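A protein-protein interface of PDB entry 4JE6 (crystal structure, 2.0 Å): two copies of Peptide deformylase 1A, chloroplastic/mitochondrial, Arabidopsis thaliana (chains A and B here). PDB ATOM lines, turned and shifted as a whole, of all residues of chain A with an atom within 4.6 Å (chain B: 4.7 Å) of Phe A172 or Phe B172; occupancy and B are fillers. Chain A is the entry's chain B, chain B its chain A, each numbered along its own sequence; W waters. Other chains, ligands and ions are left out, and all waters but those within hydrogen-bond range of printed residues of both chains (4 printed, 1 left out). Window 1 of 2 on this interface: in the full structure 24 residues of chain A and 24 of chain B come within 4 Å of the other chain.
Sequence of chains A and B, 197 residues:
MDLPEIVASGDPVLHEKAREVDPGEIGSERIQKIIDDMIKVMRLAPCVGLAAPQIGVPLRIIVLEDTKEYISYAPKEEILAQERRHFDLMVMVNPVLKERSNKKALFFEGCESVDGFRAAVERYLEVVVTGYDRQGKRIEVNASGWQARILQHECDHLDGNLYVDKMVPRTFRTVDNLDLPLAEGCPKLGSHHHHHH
Gly A10 touches Phe B172, and with the chains exchanged Phe A172 touches Gly B10.
Val A114 touches Phe B172, and with the chains exchanged Phe A172 touches Val B114.
Val A164 touches Met B167, and with the chains exchanged Met A167 touches Val B164.
Phe B172 touches its own counterpart, Phe A172.
Positions printed for both chains: 9, 10, 15, 114, 117, 118, 119, 163, 164, 167, 168, 170, 171, 172 and 173.
Among the printed residues, merely in contact across the chains: Arg A170 with His B15 (3.2 Å), His A15 with Arg B170 (3.4 Å), Ser A9 with Arg B173 (3.4 Å), Arg A173 with Gly B10 (3.4 Å), Arg A173 with Ser B9 (3.4 Å), Gly A10 with Arg B173 (3.4 Å), Phe A117 with Phe B117 (3.6 Å), Phe A172 with Gly B10 (3.6 Å), Met A167 with Val B164 (3.6 Å), Val A164 with Met B167 (3.7 Å), Phe A172 with Val B114 (3.7 Å), Gly A10 with Phe B172 (3.7 Å), Phe A172 with Phe B172 (3.8 Å), Val A164 with Phe B172 (3.9 Å), His A15 with Phe B172 (3.9 Å), Phe A172 with Val B164 (3.9 Å), Val A114 with Phe B172 (3.9 Å), Phe A172 with His B15 (3.9 Å) and Phe A117 with Val B114 (3.9 Å).
Hydrophobic or aromatic side chains of chain B within 4 Å of the printed part of chain A: His B15, Val B114, Phe B117, Val B164, Met B167 and Phe B172.
Along chain B the printed residues that touch a printed residue of chain A span positions 9 to 173.
Of the 15 printed residues of chain A, 10 touch a printed residue of chain B.
Hydrophobic or aromatic side chains of chain A within 4 Å of the printed part of chain B: His A15, Val A114, Phe A117, Val A164, Met A167 and Phe A172.
Among the printed residues, no Asp or Glu carboxylate lies within 4 Å of a Lys or Arg side-chain nitrogen of the other chain.
The backbone carbonyl oxygen (O) of Phe A172 lies within hydrogen-bond range of the side-chain hydroxyl (OG) of Ser B9, 2.7 Å away.
The side-chain hydroxyl (OG) of Ser A9 lies within hydrogen-bond range of the backbone carbonyl oxygen (O) of Phe B172, 2.7 Å away.
The side-chain hydroxyl (OG) of Ser B9 lies within hydrogen-bond range of a ring nitrogen (NE2) of His B15 (3.5 Å).
The backbone carbonyl oxygen (O) of Phe B117 is in hydrogen-bond range of the side-chain hydroxyl (OH) of Tyr B163, at 3.5 Å.
The backbone NH (N) of Arg B118 is in hydrogen-bond range of the backbone carbonyl oxygen (O) of Arg B173.
A ring nitrogen (NE2) of His A15 sits at hydrogen-bond distance from the backbone NH (N) of Gly A10, at 2.9 Å.
The backbone NH (N) of Arg A118 is in hydrogen-bond range of the backbone carbonyl oxygen (O) of Arg A173.
The guanidinium group (NE) of Arg A173 sits at hydrogen-bond distance from the backbone carbonyl oxygen (O) of Thr A171.
Water W3 bridges the backbone carbonyl oxygen of His A15 (2.5 Å) and the guanidinium group of Arg B170 (3.1 Å).
Water W1 bridges the backbone carbonyl oxygen of His B15 (2.7 Å) and the guanidinium group of Arg A170 (3.5 Å).
Water W2 lies within hydrogen-bond range of the backbone carbonyl oxygen of Gly A10 (2.7 Å) and the guanidinium group of Arg B173 (3.2 Å).
Water W4 lies within hydrogen-bond range of O of Gly B10 and NH2 of Arg A173.
Printed residues of chain B within 4 Å of Ser A9: Phe B172 and Arg B173.
Of the printed residues of chain B, His A15 touches Arg B170 (3.4 Å) and Phe B172 (3.9 Å).
Of the printed residues of chain B, Phe A117 touches Val B114 (3.9 Å) and Phe B117 (3.6 Å).
Of the printed residues of chain B, Val A164 touches Met B167 and Phe B172.
Phe A172 touches just these residues of chain B: Ser B9 (2.7 Å), Gly B10 (3.6 Å), His B15 (3.9 Å), Val B114 (3.7 Å), Val B164 (3.9 Å) and Phe B172 (3.8 Å).
Of the printed residues of chain A, Ser B9 touches Phe A172 (2.7 Å) and Arg A173 (3.4 Å).
Val B168 touches none of the printed residues of chain A.
Of the printed residues of chain A, Phe B172 touches Ser A9, Gly A10, His A15, Val A114, Val A164 and Phe A172.
The nearest printed residue of chain B that does not touch Phe A172 is Phe B117 (5.6 Å).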
ATOM      1  N   SER A   9     -20.903   9.310  34.483  1.00  0.00           N
ATOM      2  CA  SER A   9     -22.161   8.705  34.136  1.00  0.00           C
ATOM      3  C   SER A   9     -21.980   7.211  33.829  1.00  0.00           C
ATOM      4  O   SER A   9     -21.056   6.825  33.109  1.00  0.00           O
ATOM      5  CB  SER A   9     -22.805   9.447  32.942  1.00  0.00           C
ATOM      6  OG  SER A   9     -24.208   9.215  32.907  1.00  0.00           O
ATOM      7  N   GLY A  10     -22.848   6.386  34.412  1.00  0.00           N
ATOM      8  CA  GLY A  10     -22.800   4.933  34.250  1.00  0.00           C
ATOM      9  C   GLY A  10     -22.529   4.220  35.559  1.00  0.00           C
ATOM     10  O   GLY A  10     -22.945   3.070  35.758  1.00  0.00           O
ATOM     11  N   HIS A  15     -27.054   7.023  39.776  1.00  0.00           N
ATOM     12  CA  HIS A  15     -28.362   6.768  39.179  1.00  0.00           C
ATOM     13  C   HIS A  15     -29.309   6.121  40.172  1.00  0.00           C
ATOM     14  O   HIS A  15     -30.311   5.502  39.780  1.00  0.00           O
ATOM     15  CB  HIS A  15     -28.185   5.862  37.940  1.00  0.00           C
ATOM     16  CG  HIS A  15     -27.133   6.343  36.991  1.00  0.00           C
ATOM     17  ND1 HIS A  15     -27.317   7.435  36.165  1.00  0.00           N
ATOM     18  CD2 HIS A  15     -25.884   5.889  36.745  1.00  0.00           C
ATOM     19  CE1 HIS A  15     -26.223   7.631  35.452  1.00  0.00           C
ATOM     20  NE2 HIS A  15     -25.336   6.709  35.787  1.00  0.00           N
ATOM     21  N   VAL A 114     -20.652  14.315  33.365  1.00  0.00           N
ATOM     22  CA  VAL A 114     -20.888  14.171  31.905  1.00  0.00           C
ATOM     23  C   VAL A 114     -19.867  15.053  31.177  1.00  0.00           C
ATOM     24  O   VAL A 114     -20.163  16.181  30.772  1.00  0.00           O
ATOM     25  CB  VAL A 114     -22.361  14.563  31.487  1.00  0.00           C
ATOM     26  CG1 VAL A 114     -22.563  14.424  29.975  1.00  0.00           C
ATOM     27  CG2 VAL A 114     -23.403  13.722  32.254  1.00  0.00           C
ATOM     28  N   PHE A 117     -19.925  17.865  27.247  1.00  0.00           N
ATOM     29  CA  PHE A 117     -21.244  18.158  26.660  1.00  0.00           C
ATOM     30  C   PHE A 117     -22.053  19.143  27.514  1.00  0.00           C
ATOM     31  O   PHE A 117     -21.712  19.367  28.693  1.00  0.00           O
ATOM     32  CB  PHE A 117     -22.034  16.850  26.410  1.00  0.00           C
ATOM     33  CG  PHE A 117     -21.445  15.980  25.316  1.00  0.00           C
ATOM     34  CD1 PHE A 117     -20.412  15.074  25.595  1.00  0.00           C
ATOM     35  CD2 PHE A 117     -21.901  16.083  23.996  1.00  0.00           C
ATOM     36  CE1 PHE A 117     -19.850  14.281  24.586  1.00  0.00           C
ATOM     37  CE2 PHE A 117     -21.321  15.309  22.981  1.00  0.00           C
ATOM     38  CZ  PHE A 117     -20.308  14.398  23.276  1.00  0.00           C
ATOM     39  N   ARG A 118     -23.090  19.731  26.889  1.00  0.00           N
ATOM     40  CA  ARG A 118     -24.082  20.616  27.515  1.00  0.00           C
ATOM     41  C   ARG A 118     -25.430  20.370  26.845  1.00  0.00           C
ATOM     42  O   ARG A 118     -25.481  19.813  25.767  1.00  0.00           O
ATOM     43  CB  ARG A 118     -23.729  22.105  27.303  1.00  0.00           C
ATOM     44  CG  ARG A 118     -22.270  22.508  27.643  1.00  0.00           C
ATOM     45  CD  ARG A 118     -22.112  22.631  29.175  1.00  0.00           C
ATOM     46  NE  ARG A 118     -20.870  23.289  29.578  1.00  0.00           N
ATOM     47  CZ  ARG A 118     -19.769  22.654  29.976  1.00  0.00           C
ATOM     48  NH1 ARG A 118     -18.705  23.352  30.341  1.00  0.00           N
ATOM     49  NH2 ARG A 118     -19.727  21.324  30.024  1.00  0.00           N
ATOM     50  N   ALA A 119     -26.515  20.796  27.484  1.00  0.00           N
ATOM     51  CA  ALA A 119     -27.826  20.761  26.876  1.00  0.00           C
ATOM     52  C   ALA A 119     -28.677  21.842  27.531  1.00  0.00           C
ATOM     53  O   ALA A 119     -28.364  22.313  28.642  1.00  0.00           O
ATOM     54  CB  ALA A 119     -28.472  19.357  27.043  1.00  0.00           C
ATOM     55  N   TYR A 163     -29.074  15.659  34.281  1.00  0.00           N
ATOM     56  CA  TYR A 163     -29.739  16.676  33.453  1.00  0.00           C
ATOM     57  C   TYR A 163     -30.090  16.156  32.063  1.00  0.00           C
ATOM     58  O   TYR A 163     -31.029  16.647  31.432  1.00  0.00           O
ATOM     59  CB  TYR A 163     -28.891  17.960  33.331  1.00  0.00           C
ATOM     60  CG  TYR A 163     -27.726  17.857  32.366  1.00  0.00           C
ATOM     61  CD1 TYR A 163     -26.438  17.482  32.822  1.00  0.00           C
ATOM     62  CD2 TYR A 163     -27.890  18.155  31.001  1.00  0.00           C
ATOM     63  CE1 TYR A 163     -25.331  17.404  31.936  1.00  0.00           C
ATOM     64  CE2 TYR A 163     -26.789  18.067  30.105  1.00  0.00           C
ATOM     65  CZ  TYR A 163     -25.517  17.703  30.583  1.00  0.00           C
ATOM     66  OH  TYR A 163     -24.450  17.612  29.707  1.00  0.00           O
ATOM     67  N   VAL A 164     -29.327  15.171  31.594  1.00  0.00           N
ATOM     68  CA  VAL A 164     -29.540  14.597  30.252  1.00  0.00           C
ATOM     69  C   VAL A 164     -30.909  13.906  30.103  1.00  0.00           C
ATOM     70  O   VAL A 164     -31.377  13.713  28.980  1.00  0.00           O
ATOM     71  CB  VAL A 164     -28.400  13.616  29.828  1.00  0.00           C
ATOM     72  CG1 VAL A 164     -27.049  14.362  29.704  1.00  0.00           C
ATOM     73  CG2 VAL A 164     -28.296  12.389  30.800  1.00  0.00           C
ATOM     74  N   MET A 167     -33.612  17.160  29.479  1.00  0.00           N
ATOM     75  CA  MET A 167     -33.102  18.269  28.647  1.00  0.00           C
ATOM     76  C   MET A 167     -34.075  18.519  27.507  1.00  0.00           C
ATOM     77  O   MET A 167     -34.824  17.616  27.109  1.00  0.00           O
ATOM     78  CB  MET A 167     -31.700  17.957  28.105  1.00  0.00           C
ATOM     79  CG  MET A 167     -31.620  16.688  27.234  1.00  0.00           C
ATOM     80  SD  MET A 167     -29.888  16.314  26.901  1.00  0.00           S
ATOM     81  CE  MET A 167     -30.030  14.705  26.069  1.00  0.00           C
ATOM     82  N   VAL A 168     -34.074  19.737  26.981  1.00  0.00           N
ATOM     83  CA  VAL A 168     -34.935  20.078  25.839  1.00  0.00           C
ATOM     84  C   VAL A 168     -34.402  19.290  24.618  1.00  0.00           C
ATOM     85  O   VAL A 168     -33.188  19.308  24.368  1.00  0.00           O
ATOM     86  CB  VAL A 168     -34.879  21.600  25.558  1.00  0.00           C
ATOM     87  CG1 VAL A 168     -35.555  21.957  24.217  1.00  0.00           C
ATOM     88  CG2 VAL A 168     -35.535  22.390  26.739  1.00  0.00           C
ATOM     89  N   ARG A 170     -33.126  18.087  21.040  1.00  0.00           N
ATOM     90  CA  ARG A 170     -32.348  18.712  19.972  1.00  0.00           C
ATOM     91  C   ARG A 170     -31.412  19.813  20.445  1.00  0.00           C
ATOM     92  O   ARG A 170     -30.934  20.606  19.615  1.00  0.00           O
ATOM     93  CB  ARG A 170     -33.243  19.212  18.828  1.00  0.00           C
ATOM     94  CG  ARG A 170     -34.064  18.076  18.243  1.00  0.00           C
ATOM     95  CD  ARG A 170     -34.820  18.447  16.988  1.00  0.00           C
ATOM     96  NE  ARG A 170     -35.655  17.326  16.580  1.00  0.00           N
ATOM     97  CZ  ARG A 170     -36.881  17.435  16.092  1.00  0.00           C
ATOM     98  NH1 ARG A 170     -37.566  16.344  15.780  1.00  0.00           N
ATOM     99  NH2 ARG A 170     -37.435  18.636  15.939  1.00  0.00           N
ATOM    100  N   THR A 171     -31.106  19.846  21.746  1.00  0.00           N
ATOM    101  CA  THR A 171     -30.168  20.878  22.262  1.00  0.00           C
ATOM    102  C   THR A 171     -28.852  20.326  22.793  1.00  0.00           C
ATOM    103  O   THR A 171     -27.883  21.076  22.952  1.00  0.00           O
ATOM    104  CB  THR A 171     -30.786  21.776  23.357  1.00  0.00           C
ATOM    105  OG1 THR A 171     -30.923  21.031  24.582  1.00  0.00           O
ATOM    106  CG2 THR A 171     -32.136  22.355  22.914  1.00  0.00           C
ATOM    107  N   PHE A 172     -28.814  19.020  23.044  1.00  0.00           N
ATOM    108  CA  PHE A 172     -27.601  18.348  23.515  1.00  0.00           C
ATOM    109  C   PHE A 172     -26.444  18.632  22.530  1.00  0.00           C
ATOM    110  O   PHE A 172     -26.616  18.577  21.312  1.00  0.00           O
ATOM    111  CB  PHE A 172     -27.884  16.843  23.669  1.00  0.00           C
ATOM    112  CG  PHE A 172     -26.756  16.053  24.246  1.00  0.00           C
ATOM    113  CD1 PHE A 172     -25.949  15.275  23.417  1.00  0.00           C
ATOM    114  CD2 PHE A 172     -26.506  16.062  25.626  1.00  0.00           C
ATOM    115  CE1 PHE A 172     -24.906  14.514  23.942  1.00  0.00           C
ATOM    116  CE2 PHE A 172     -25.462  15.299  26.165  1.00  0.00           C
ATOM    117  CZ  PHE A 172     -24.662  14.513  25.316  1.00  0.00           C
ATOM    118  N   ARG A 173     -25.270  18.954  23.064  1.00  0.00           N
ATOM    119  CA  ARG A 173     -24.185  19.402  22.207  1.00  0.00           C
ATOM    120  C   ARG A 173     -22.844  19.308  22.897  1.00  0.00           C
ATOM    121  O   ARG A 173     -22.757  19.297  24.133  1.00  0.00           O
ATOM    122  CB  ARG A 173     -24.430  20.858  21.771  1.00  0.00           C
ATOM    123  CG  ARG A 173     -24.524  21.862  22.956  1.00  0.00           C
ATOM    124  CD  ARG A 173     -24.922  23.228  22.442  1.00  0.00           C
ATOM    125  NE  ARG A 173     -26.126  23.220  21.607  1.00  0.00           N
ATOM    126  CZ  ARG A 173     -26.475  24.216  20.781  1.00  0.00           C
ATOM    127  NH1 ARG A 173     -25.720  25.319  20.659  1.00  0.00           N
ATOM    128  NH2 ARG A 173     -27.585  24.111  20.080  1.00  0.00           N
ATOM    129  N   SER B   9     -22.783  16.661  17.631  1.00  0.00           N
ATOM    130  CA  SER B   9     -23.968  17.238  18.283  1.00  0.00           C
ATOM    131  C   SER B   9     -23.786  18.733  18.611  1.00  0.00           C
ATOM    132  O   SER B   9     -22.736  19.150  19.119  1.00  0.00           O
ATOM    133  CB  SER B   9     -24.294  16.425  19.551  1.00  0.00           C
ATOM    134  OG  SER B   9     -25.666  16.496  19.849  1.00  0.00           O
ATOM    135  N   GLY B  10     -24.813  19.528  18.305  1.00  0.00           N
ATOM    136  CA  GLY B  10     -24.725  20.986  18.386  1.00  0.00           C
ATOM    137  C   GLY B  10     -24.874  21.679  17.040  1.00  0.00           C
ATOM    138  O   GLY B  10     -25.463  22.787  16.952  1.00  0.00           O
ATOM    139  N   HIS B  15     -29.879  18.329  13.673  1.00  0.00           N
ATOM    140  CA  HIS B  15     -31.044  18.523  14.543  1.00  0.00           C
ATOM    141  C   HIS B  15     -32.243  19.088  13.786  1.00  0.00           C
ATOM    142  O   HIS B  15     -33.208  19.532  14.398  1.00  0.00           O
ATOM    143  CB  HIS B  15     -30.656  19.460  15.707  1.00  0.00           C
ATOM    144  CG  HIS B  15     -29.495  18.955  16.513  1.00  0.00           C
ATOM    145  ND1 HIS B  15     -28.264  19.585  16.539  1.00  0.00           N
ATOM    146  CD2 HIS B  15     -29.375  17.864  17.304  1.00  0.00           C
ATOM    147  CE1 HIS B  15     -27.439  18.902  17.311  1.00  0.00           C
ATOM    148  NE2 HIS B  15     -28.094  17.864  17.802  1.00  0.00           N
ATOM    149  N   VAL B 114     -21.945  11.717  18.873  1.00  0.00           N
ATOM    150  CA  VAL B 114     -21.863  11.889  20.341  1.00  0.00           C
ATOM    151  C   VAL B 114     -20.698  11.019  20.815  1.00  0.00           C
ATOM    152  O   VAL B 114     -20.890   9.869  21.233  1.00  0.00           O
ATOM    153  CB  VAL B 114     -23.168  11.456  21.078  1.00  0.00           C
ATOM    154  CG1 VAL B 114     -23.042  11.631  22.630  1.00  0.00           C
ATOM    155  CG2 VAL B 114     -24.408  12.213  20.530  1.00  0.00           C
ATOM    156  N   PHE B 117     -19.963   8.225  24.621  1.00  0.00           N
ATOM    157  CA  PHE B 117     -21.121   7.851  25.432  1.00  0.00           C
ATOM    158  C   PHE B 117     -21.967   6.782  24.774  1.00  0.00           C
ATOM    159  O   PHE B 117     -21.852   6.533  23.569  1.00  0.00           O
ATOM    160  CB  PHE B 117     -21.957   9.107  25.812  1.00  0.00           C
ATOM    161  CG  PHE B 117     -21.232  10.034  26.765  1.00  0.00           C
ATOM    162  CD1 PHE B 117     -21.368   9.882  28.143  1.00  0.00           C
ATOM    163  CD2 PHE B 117     -20.372  11.013  26.286  1.00  0.00           C
ATOM    164  CE1 PHE B 117     -20.673  10.707  29.028  1.00  0.00           C
ATOM    165  CE2 PHE B 117     -19.680  11.855  27.175  1.00  0.00           C
ATOM    166  CZ  PHE B 117     -19.823  11.692  28.538  1.00  0.00           C
ATOM    167  N   ARG B 118     -22.775   6.115  25.596  1.00  0.00           N
ATOM    168  CA  ARG B 118     -23.774   5.143  25.145  1.00  0.00           C
ATOM    169  C   ARG B 118     -25.032   5.322  26.007  1.00  0.00           C
ATOM    170  O   ARG B 118     -24.969   5.887  27.102  1.00  0.00           O
ATOM    171  CB  ARG B 118     -23.254   3.696  25.346  1.00  0.00           C
ATOM    172  CG  ARG B 118     -21.916   3.374  24.679  1.00  0.00           C
ATOM    173  CD  ARG B 118     -22.134   3.132  23.165  1.00  0.00           C
ATOM    174  NE  ARG B 118     -20.910   2.656  22.518  1.00  0.00           N
ATOM    175  CZ  ARG B 118     -19.970   3.436  21.999  1.00  0.00           C
ATOM    176  NH1 ARG B 118     -20.107   4.760  22.008  1.00  0.00           N
ATOM    177  NH2 ARG B 118     -18.875   2.889  21.467  1.00  0.00           N
ATOM    178  N   ALA B 119     -26.164   4.827  25.515  1.00  0.00           N
ATOM    179  CA  ALA B 119     -27.352   4.684  26.340  1.00  0.00           C
ATOM    180  C   ALA B 119     -28.279   3.599  25.773  1.00  0.00           C
ATOM    181  O   ALA B 119     -28.151   3.183  24.625  1.00  0.00           O
ATOM    182  CB  ALA B 119     -28.075   6.044  26.511  1.00  0.00           C
ATOM    183  N   TYR B 163     -30.337   9.664  19.341  1.00  0.00           N
ATOM    184  CA  TYR B 163     -30.749   8.700  20.362  1.00  0.00           C
ATOM    185  C   TYR B 163     -30.890   9.296  21.779  1.00  0.00           C
ATOM    186  O   TYR B 163     -31.675   8.793  22.601  1.00  0.00           O
ATOM    187  CB  TYR B 163     -29.820   7.484  20.362  1.00  0.00           C
ATOM    188  CG  TYR B 163     -28.507   7.679  21.085  1.00  0.00           C
ATOM    189  CD1 TYR B 163     -28.385   7.363  22.439  1.00  0.00           C
ATOM    190  CD2 TYR B 163     -27.380   8.161  20.415  1.00  0.00           C
ATOM    191  CE1 TYR B 163     -27.176   7.535  23.117  1.00  0.00           C
ATOM    192  CE2 TYR B 163     -26.166   8.332  21.082  1.00  0.00           C
ATOM    193  CZ  TYR B 163     -26.075   8.005  22.426  1.00  0.00           C
ATOM    194  OH  TYR B 163     -24.891   8.155  23.096  1.00  0.00           O
ATOM    195  N   VAL B 164     -30.123  10.349  22.060  1.00  0.00           N
ATOM    196  CA  VAL B 164     -30.065  10.902  23.414  1.00  0.00           C
ATOM    197  C   VAL B 164     -31.407  11.486  23.829  1.00  0.00           C
ATOM    198  O   VAL B 164     -31.670  11.638  25.010  1.00  0.00           O
ATOM    199  CB  VAL B 164     -28.917  11.946  23.599  1.00  0.00           C
ATOM    200  CG1 VAL B 164     -27.525  11.257  23.443  1.00  0.00           C
ATOM    201  CG2 VAL B 164     -29.087  13.145  22.645  1.00  0.00           C
ATOM    202  N   MET B 167     -33.764   8.000  24.927  1.00  0.00           N
ATOM    203  CA  MET B 167     -33.082   6.947  25.672  1.00  0.00           C
ATOM    204  C   MET B 167     -33.804   6.660  26.986  1.00  0.00           C
ATOM    205  O   MET B 167     -34.514   7.518  27.524  1.00  0.00           O
ATOM    206  CB  MET B 167     -31.606   7.322  25.930  1.00  0.00           C
ATOM    207  CG  MET B 167     -31.403   8.565  26.806  1.00  0.00           C
ATOM    208  SD  MET B 167     -29.683   9.116  26.763  1.00  0.00           S
ATOM    209  CE  MET B 167     -29.821  10.646  27.727  1.00  0.00           C
ATOM    210  N   VAL B 168     -33.652   5.437  27.483  1.00  0.00           N
ATOM    211  CA  VAL B 168     -34.212   5.028  28.759  1.00  0.00           C
ATOM    212  C   VAL B 168     -33.501   5.840  29.862  1.00  0.00           C
ATOM    213  O   VAL B 168     -32.276   5.905  29.861  1.00  0.00           O
ATOM    214  CB  VAL B 168     -33.989   3.515  28.983  1.00  0.00           C
ATOM    215  CG1 VAL B 168     -34.385   3.126  30.404  1.00  0.00           C
ATOM    216  CG2 VAL B 168     -34.842   2.693  28.001  1.00  0.00           C
ATOM    217  N   ARG B 170     -31.644   7.112  33.127  1.00  0.00           N
ATOM    218  CA  ARG B 170     -30.613   6.566  34.017  1.00  0.00           C
ATOM    219  C   ARG B 170     -29.699   5.522  33.388  1.00  0.00           C
ATOM    220  O   ARG B 170     -28.990   4.834  34.101  1.00  0.00           O
ATOM    221  CB  ARG B 170     -31.214   6.027  35.328  1.00  0.00           C
ATOM    222  CG  ARG B 170     -32.149   7.024  35.972  1.00  0.00           C
ATOM    223  CD  ARG B 170     -32.383   6.767  37.449  1.00  0.00           C
ATOM    224  NE  ARG B 170     -33.345   7.763  37.912  1.00  0.00           N
ATOM    225  CZ  ARG B 170     -34.230   7.571  38.869  1.00  0.00           C
ATOM    226  NH1 ARG B 170     -35.072   8.542  39.195  1.00  0.00           N
ATOM    227  NH2 ARG B 170     -34.266   6.409  39.505  1.00  0.00           N
ATOM    228  N   THR B 171     -29.671   5.447  32.060  1.00  0.00           N
ATOM    229  CA  THR B 171     -28.792   4.503  31.363  1.00  0.00           C
ATOM    230  C   THR B 171     -27.650   5.170  30.599  1.00  0.00           C
ATOM    231  O   THR B 171     -26.729   4.488  30.190  1.00  0.00           O
ATOM    232  CB  THR B 171     -29.585   3.604  30.381  1.00  0.00           C
ATOM    233  OG1 THR B 171     -30.031   4.396  29.282  1.00  0.00           O
ATOM    234  CG2 THR B 171     -30.794   2.955  31.084  1.00  0.00           C
ATOM    235  N   PHE B 172     -27.717   6.488  30.399  1.00  0.00           N
ATOM    236  CA  PHE B 172     -26.645   7.239  29.748  1.00  0.00           C
ATOM    237  C   PHE B 172     -25.337   7.005  30.504  1.00  0.00           C
ATOM    238  O   PHE B 172     -25.306   7.035  31.745  1.00  0.00           O
ATOM    239  CB  PHE B 172     -27.000   8.733  29.712  1.00  0.00           C
ATOM    240  CG  PHE B 172     -26.092   9.576  28.838  1.00  0.00           C
ATOM    241  CD1 PHE B 172     -26.126   9.453  27.446  1.00  0.00           C
ATOM    242  CD2 PHE B 172     -25.229  10.512  29.410  1.00  0.00           C
ATOM    243  CE1 PHE B 172     -25.321  10.256  26.642  1.00  0.00           C
ATOM    244  CE2 PHE B 172     -24.407  11.313  28.594  1.00  0.00           C
ATOM    245  CZ  PHE B 172     -24.473  11.185  27.222  1.00  0.00           C
ATOM    246  N   ARG B 173     -24.270   6.743  29.762  1.00  0.00           N
ATOM    247  CA  ARG B 173     -22.999   6.314  30.389  1.00  0.00           C
ATOM    248  C   ARG B 173     -21.807   6.521  29.475  1.00  0.00           C
ATOM    249  O   ARG B 173     -21.958   6.547  28.253  1.00  0.00           O
ATOM    250  CB  ARG B 173     -23.064   4.841  30.827  1.00  0.00           C
ATOM    251  CG  ARG B 173     -23.428   3.863  29.711  1.00  0.00           C
ATOM    252  CD  ARG B 173     -23.637   2.458  30.285  1.00  0.00           C
ATOM    253  NE  ARG B 173     -24.665   2.495  31.329  1.00  0.00           N
ATOM    254  CZ  ARG B 173     -24.839   1.570  32.265  1.00  0.00           C
ATOM    255  NH1 ARG B 173     -24.075   0.497  32.298  1.00  0.00           N
ATOM    256  NH2 ARG B 173     -25.779   1.736  33.184  1.00  0.00           N
HETATM  257  O   HOH W   1     -35.526  20.808  14.020  1.00  0.00           O
HETATM  258  O   HOH W   2     -25.459   2.346  36.325  1.00  0.00           O
HETATM  259  O   HOH W   3     -32.334   4.252  40.622  1.00  0.00           O
HETATM  260  O   HOH W   4     -28.225  23.252  16.804  1.00  0.00           O
